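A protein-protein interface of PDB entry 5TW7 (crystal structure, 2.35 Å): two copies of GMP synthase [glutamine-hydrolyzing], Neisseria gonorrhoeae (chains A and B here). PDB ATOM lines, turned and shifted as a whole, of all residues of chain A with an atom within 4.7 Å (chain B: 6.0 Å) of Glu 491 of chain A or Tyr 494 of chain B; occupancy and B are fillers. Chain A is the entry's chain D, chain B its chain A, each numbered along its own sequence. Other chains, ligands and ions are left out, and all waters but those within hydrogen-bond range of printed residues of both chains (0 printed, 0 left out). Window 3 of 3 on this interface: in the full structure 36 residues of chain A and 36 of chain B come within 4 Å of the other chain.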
ATOM      1  N   TRP A 444       3.038 -19.624  33.929  1.00  0.00           N
ATOM      2  CA  TRP A 444       3.821 -18.553  33.319  1.00  0.00           C
ATOM      3  C   TRP A 444       3.293 -17.182  33.720  1.00  0.00           C
ATOM      4  O   TRP A 444       4.059 -16.210  33.708  1.00  0.00           O
ATOM      5  CB  TRP A 444       3.891 -18.721  31.777  1.00  0.00           C
ATOM      6  CG  TRP A 444       4.939 -19.754  31.391  1.00  0.00           C
ATOM      7  CD1 TRP A 444       4.734 -21.083  31.113  1.00  0.00           C
ATOM      8  CD2 TRP A 444       6.360 -19.554  31.339  1.00  0.00           C
ATOM      9  NE1 TRP A 444       5.938 -21.709  30.862  1.00  0.00           N
ATOM     10  CE2 TRP A 444       6.949 -20.796  31.005  1.00  0.00           C
ATOM     11  CE3 TRP A 444       7.190 -18.442  31.531  1.00  0.00           C
ATOM     12  CZ2 TRP A 444       8.326 -20.951  30.854  1.00  0.00           C
ATOM     13  CZ3 TRP A 444       8.544 -18.598  31.393  1.00  0.00           C
ATOM     14  CH2 TRP A 444       9.105 -19.841  31.050  1.00  0.00           C
ATOM     15  N   TRP A 489      13.216  -9.712  29.250  1.00  0.00           N
ATOM     16  CA  TRP A 489      11.964 -10.195  28.689  1.00  0.00           C
ATOM     17  C   TRP A 489      11.849 -11.702  28.906  1.00  0.00           C
ATOM     18  O   TRP A 489      12.844 -12.432  28.917  1.00  0.00           O
ATOM     19  CB  TRP A 489      11.849  -9.835  27.204  1.00  0.00           C
ATOM     20  CG  TRP A 489      12.994 -10.269  26.313  1.00  0.00           C
ATOM     21  CD1 TRP A 489      14.134  -9.567  26.033  1.00  0.00           C
ATOM     22  CD2 TRP A 489      13.073 -11.483  25.545  1.00  0.00           C
ATOM     23  NE1 TRP A 489      14.928 -10.281  25.161  1.00  0.00           N
ATOM     24  CE2 TRP A 489      14.291 -11.449  24.831  1.00  0.00           C
ATOM     25  CE3 TRP A 489      12.229 -12.592  25.391  1.00  0.00           C
ATOM     26  CZ2 TRP A 489      14.688 -12.481  23.978  1.00  0.00           C
ATOM     27  CZ3 TRP A 489      12.616 -13.606  24.540  1.00  0.00           C
ATOM     28  CH2 TRP A 489      13.843 -13.549  23.848  1.00  0.00           C
ATOM     29  N   ALA A 490      10.624 -12.159  29.131  1.00  0.00           N
ATOM     30  CA  ALA A 490      10.421 -13.547  29.523  1.00  0.00           C
ATOM     31  C   ALA A 490      10.647 -14.468  28.324  1.00  0.00           C
ATOM     32  O   ALA A 490      10.164 -14.205  27.223  1.00  0.00           O
ATOM     33  CB  ALA A 490       9.015 -13.734  30.090  1.00  0.00           C
ATOM     34  N   GLU A 491      11.400 -15.546  28.543  1.00  0.00           N
ATOM     35  CA  GLU A 491      11.631 -16.570  27.531  1.00  0.00           C
ATOM     36  C   GLU A 491      10.439 -17.522  27.530  1.00  0.00           C
ATOM     37  O   GLU A 491      10.524 -18.696  27.891  1.00  0.00           O
ATOM     38  CB  GLU A 491      12.959 -17.277  27.785  1.00  0.00           C
ATOM     39  CG  GLU A 491      14.087 -16.255  27.735  1.00  0.00           C
ATOM     40  CD  GLU A 491      15.464 -16.845  27.775  1.00  0.00           C
ATOM     41  OE1 GLU A 491      15.604 -18.081  27.919  1.00  0.00           O
ATOM     42  OE2 GLU A 491      16.412 -16.045  27.646  1.00  0.00           O
ATOM     43  N   LEU A 492       9.305 -16.959  27.145  1.00  0.00           N
ATOM     44  CA  LEU A 492       8.068 -17.710  27.067  1.00  0.00           C
ATOM     45  C   LEU A 492       8.247 -18.864  26.089  1.00  0.00           C
ATOM     46  O   LEU A 492       8.937 -18.710  25.075  1.00  0.00           O
ATOM     47  CB  LEU A 492       6.924 -16.798  26.608  1.00  0.00           C
ATOM     48  CG  LEU A 492       6.620 -15.589  27.487  1.00  0.00           C
ATOM     49  CD1 LEU A 492       5.535 -14.719  26.887  1.00  0.00           C
ATOM     50  CD2 LEU A 492       6.205 -16.067  28.893  1.00  0.00           C
ATOM     51  N   PRO A 493       7.667 -20.027  26.374  1.00  0.00           N
ATOM     52  CA  PRO A 493       7.750 -21.144  25.425  1.00  0.00           C
ATOM     53  C   PRO A 493       7.183 -20.746  24.070  1.00  0.00           C
ATOM     54  O   PRO A 493       6.175 -20.038  23.975  1.00  0.00           O
ATOM     55  CB  PRO A 493       6.909 -22.248  26.086  1.00  0.00           C
ATOM     56  CG  PRO A 493       6.849 -21.879  27.542  1.00  0.00           C
ATOM     57  CD  PRO A 493       6.922 -20.367  27.599  1.00  0.00           C
ATOM     58  N   TYR A 494       7.856 -21.201  23.016  1.00  0.00           N
ATOM     59  CA  TYR A 494       7.426 -20.876  21.659  1.00  0.00           C
ATOM     60  C   TYR A 494       5.979 -21.300  21.426  1.00  0.00           C
ATOM     61  O   TYR A 494       5.193 -20.566  20.807  1.00  0.00           O
ATOM     62  CB  TYR A 494       8.353 -21.555  20.651  1.00  0.00           C
ATOM     63  CG  TYR A 494       9.814 -21.164  20.778  1.00  0.00           C
ATOM     64  CD1 TYR A 494      10.236 -19.866  20.486  1.00  0.00           C
ATOM     65  CD2 TYR A 494      10.782 -22.103  21.157  1.00  0.00           C
ATOM     66  CE1 TYR A 494      11.563 -19.505  20.583  1.00  0.00           C
ATOM     67  CE2 TYR A 494      12.134 -21.744  21.252  1.00  0.00           C
ATOM     68  CZ  TYR A 494      12.505 -20.440  20.952  1.00  0.00           C
ATOM     69  OH  TYR A 494      13.822 -20.062  21.034  1.00  0.00           O
ATOM     70  N   LEU B 492      13.493 -19.027  16.781  1.00  0.00           N
ATOM     71  CA  LEU B 492      14.843 -18.507  16.912  1.00  0.00           C
ATOM     72  C   LEU B 492      15.285 -18.598  18.373  1.00  0.00           C
ATOM     73  O   LEU B 492      14.467 -18.397  19.279  1.00  0.00           O
ATOM     74  CB  LEU B 492      14.892 -17.051  16.429  1.00  0.00           C
ATOM     75  CG  LEU B 492      14.515 -16.747  14.977  1.00  0.00           C
ATOM     76  CD1 LEU B 492      14.561 -15.250  14.698  1.00  0.00           C
ATOM     77  CD2 LEU B 492      15.419 -17.530  13.997  1.00  0.00           C
ATOM     78  N   PRO B 493      16.552 -18.930  18.639  1.00  0.00           N
ATOM     79  CA  PRO B 493      17.024 -18.983  20.034  1.00  0.00           C
ATOM     80  C   PRO B 493      16.825 -17.645  20.733  1.00  0.00           C
ATOM     81  O   PRO B 493      17.027 -16.583  20.142  1.00  0.00           O
ATOM     82  CB  PRO B 493      18.513 -19.333  19.909  1.00  0.00           C
ATOM     83  CG  PRO B 493      18.666 -19.953  18.526  1.00  0.00           C
ATOM     84  CD  PRO B 493      17.599 -19.290  17.661  1.00  0.00           C
ATOM     85  N   TYR B 494      16.415 -17.714  22.007  1.00  0.00           N
ATOM     86  CA  TYR B 494      16.160 -16.505  22.786  1.00  0.00           C
ATOM     87  C   TYR B 494      17.381 -15.592  22.811  1.00  0.00           C
ATOM     88  O   TYR B 494      17.256 -14.369  22.644  1.00  0.00           O
ATOM     89  CB  TYR B 494      15.752 -16.889  24.211  1.00  0.00           C
ATOM     90  CG  TYR B 494      14.498 -17.750  24.289  1.00  0.00           C
ATOM     91  CD1 TYR B 494      13.258 -17.224  23.959  1.00  0.00           C
ATOM     92  CD2 TYR B 494      14.558 -19.094  24.678  1.00  0.00           C
ATOM     93  CE1 TYR B 494      12.104 -17.999  24.008  1.00  0.00           C
ATOM     94  CE2 TYR B 494      13.406 -19.877  24.733  1.00  0.00           C
ATOM     95  CZ  TYR B 494      12.180 -19.310  24.399  1.00  0.00           C
ATOM     96  OH  TYR B 494      11.024 -20.043  24.436  1.00  0.00           O
ATOM     97  N   SER B 495      18.570 -16.165  23.006  1.00  0.00           N
ATOM     98  CA  SER B 495      19.782 -15.355  23.043  1.00  0.00           C
ATOM     99  C   SER B 495      20.058 -14.693  21.694  1.00  0.00           C
ATOM    100  O   SER B 495      20.603 -13.586  21.650  1.00  0.00           O
ATOM    101  CB  SER B 495      20.967 -16.205  23.505  1.00  0.00           C
ATOM    102  OG  SER B 495      21.038 -17.425  22.789  1.00  0.00           O
ATOM    103  N   LEU B 496      19.702 -15.344  20.589  1.00  0.00           N
ATOM    104  CA  LEU B 496      19.813 -14.682  19.290  1.00  0.00           C
ATOM    105  C   LEU B 496      18.871 -13.483  19.215  1.00  0.00           C
ATOM    106  O   LEU B 496      19.286 -12.376  18.841  1.00  0.00           O
ATOM    107  CB  LEU B 496      19.536 -15.671  18.151  1.00  0.00           C
ATOM    108  CG  LEU B 496      19.702 -15.178  16.699  1.00  0.00           C
ATOM    109  CD1 LEU B 496      20.014 -16.347  15.775  1.00  0.00           C
ATOM    110  CD2 LEU B 496      18.468 -14.436  16.186  1.00  0.00           C
ATOM    111  N   LEU B 497      17.600 -13.680  19.585  1.00  0.00           N
ATOM    112  CA  LEU B 497      16.656 -12.563  19.624  1.00  0.00           C
ATOM    113  C   LEU B 497      17.144 -11.454  20.550  1.00  0.00           C
ATOM    114  O   LEU B 497      17.121 -10.271  20.183  1.00  0.00           O
ATOM    115  CB  LEU B 497      15.268 -13.060  20.057  1.00  0.00           C
ATOM    116  CG  LEU B 497      14.566 -13.989  19.054  1.00  0.00           C
ATOM    117  CD1 LEU B 497      13.429 -14.811  19.657  1.00  0.00           C
ATOM    118  CD2 LEU B 497      14.032 -13.155  17.922  1.00  0.00           C
ATOM    119  N   GLY B 498      17.624 -11.819  21.740  1.00  0.00           N
ATOM    120  CA  GLY B 498      18.065 -10.811  22.690  1.00  0.00           C
ATOM    121  C   GLY B 498      19.260 -10.021  22.187  1.00  0.00           C
ATOM    122  O   GLY B 498      19.326  -8.798  22.348  1.00  0.00           O
ATOM    123  N   ARG B 499      20.216 -10.708  21.555  1.00  0.00           N
ATOM    124  CA  ARG B 499      21.401 -10.028  21.053  1.00  0.00           C
ATOM    125  C   ARG B 499      21.048  -9.104  19.888  1.00  0.00           C
ATOM    126  O   ARG B 499      21.556  -7.980  19.802  1.00  0.00           O
ATOM    127  CB  ARG B 499      22.436 -11.073  20.646  1.00  0.00           C
ATOM    128  CG  ARG B 499      23.851 -10.553  20.427  1.00  0.00           C
ATOM    129  CD  ARG B 499      24.822 -11.725  20.213  1.00  0.00           C
ATOM    130  NE  ARG B 499      24.343 -12.695  19.215  1.00  0.00           N
ATOM    131  CZ  ARG B 499      23.910 -13.934  19.467  1.00  0.00           C
ATOM    132  NH1 ARG B 499      23.519 -14.710  18.465  1.00  0.00           N
ATOM    133  NH2 ARG B 499      23.887 -14.416  20.702  1.00  0.00           N
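The backbone carbonyl oxygen (O) of Leu 492 of chain B lies within hydrogen-bond range of the side-chain hydroxyl (OH) of Tyr 494 of chain A (2.5 Å).
OH of Tyr 494 of chain B is in hydrogen-bond range of O of Leu 492 of chain A, 2.6 Å away.
Leu 492 of chain A touches Tyr 494 of chain B, and with the chains exchanged Tyr 494 of chain A touches Leu 492 of chain B.
Pro 493 of chain A touches Tyr 494 of chain B, and with the chains exchanged Tyr 494 of chain A touches Pro 493 of chain B.
Tyr 494 of chain B touches its own counterpart, Tyr 494 of chain A.
Positions printed for both chains: 492, 493 and 494.
CZ2 of Trp 489 of chain A touches O of Tyr 494 of chain B, at 3.5 Å.
Gly 498 of chain B touches Trp 489 of chain A (N to CZ2, 3.8 Å).
Glu 491 of chain A touches Tyr 494 of chain B.
Tyr 494 of chain B touches Pro 493 of chain A (OH to CA, 3.6 Å).
CA of Pro 493 of chain B touches OH of Tyr 494 of chain A, at 3.5 Å.
Tyr 494 of chain B touches Tyr 494 of chain A (N to OH, 3.6 Å).
Of the printed residues of chain B, Trp 489 of chain A touches Tyr 494 and Gly 498.
Glu 491 of chain A touches one residue of chain B.
Of the printed residues of chain B, Leu 492 of chain A touches Tyr 494 (2.6 Å).
Of the printed residues of chain B, Pro 493 of chain A touches Tyr 494.
Of the printed residues of chain B, Tyr 494 of chain A touches Leu 492, Pro 493 and Tyr 494.
Tyr 494 of chain B touches five residues of chain A.
Of the printed residues of chain A, Gly 498 of chain B touches Trp 489.
The nearest residue of chain B that does not touch Glu 491 of chain A is Ser 495 of chain B (5.1 Å).
The nearest printed residue of chain A that does not touch Tyr 494 of chain B is Ala 490 of chain A (5.3 Å).
The nearest printed residue of chain B that does not touch Leu 492 of chain A is Leu 492 of chain B (8.0 Å).
Of the 7 printed residues of chain A, 5 touch a printed residue of chain B.
Hydrophobic or aromatic side chains of chain A that line the printed part of chain B: Trp 489 and Tyr 494.
Hydrophobic or aromatic side chains of chain B within 4 Å of the printed part of chain A: Tyr 494.
Among the printed residues, no Asp or Glu carboxylate lies within 4 Å of a Lys or Arg side-chain nitrogen of the other chain.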
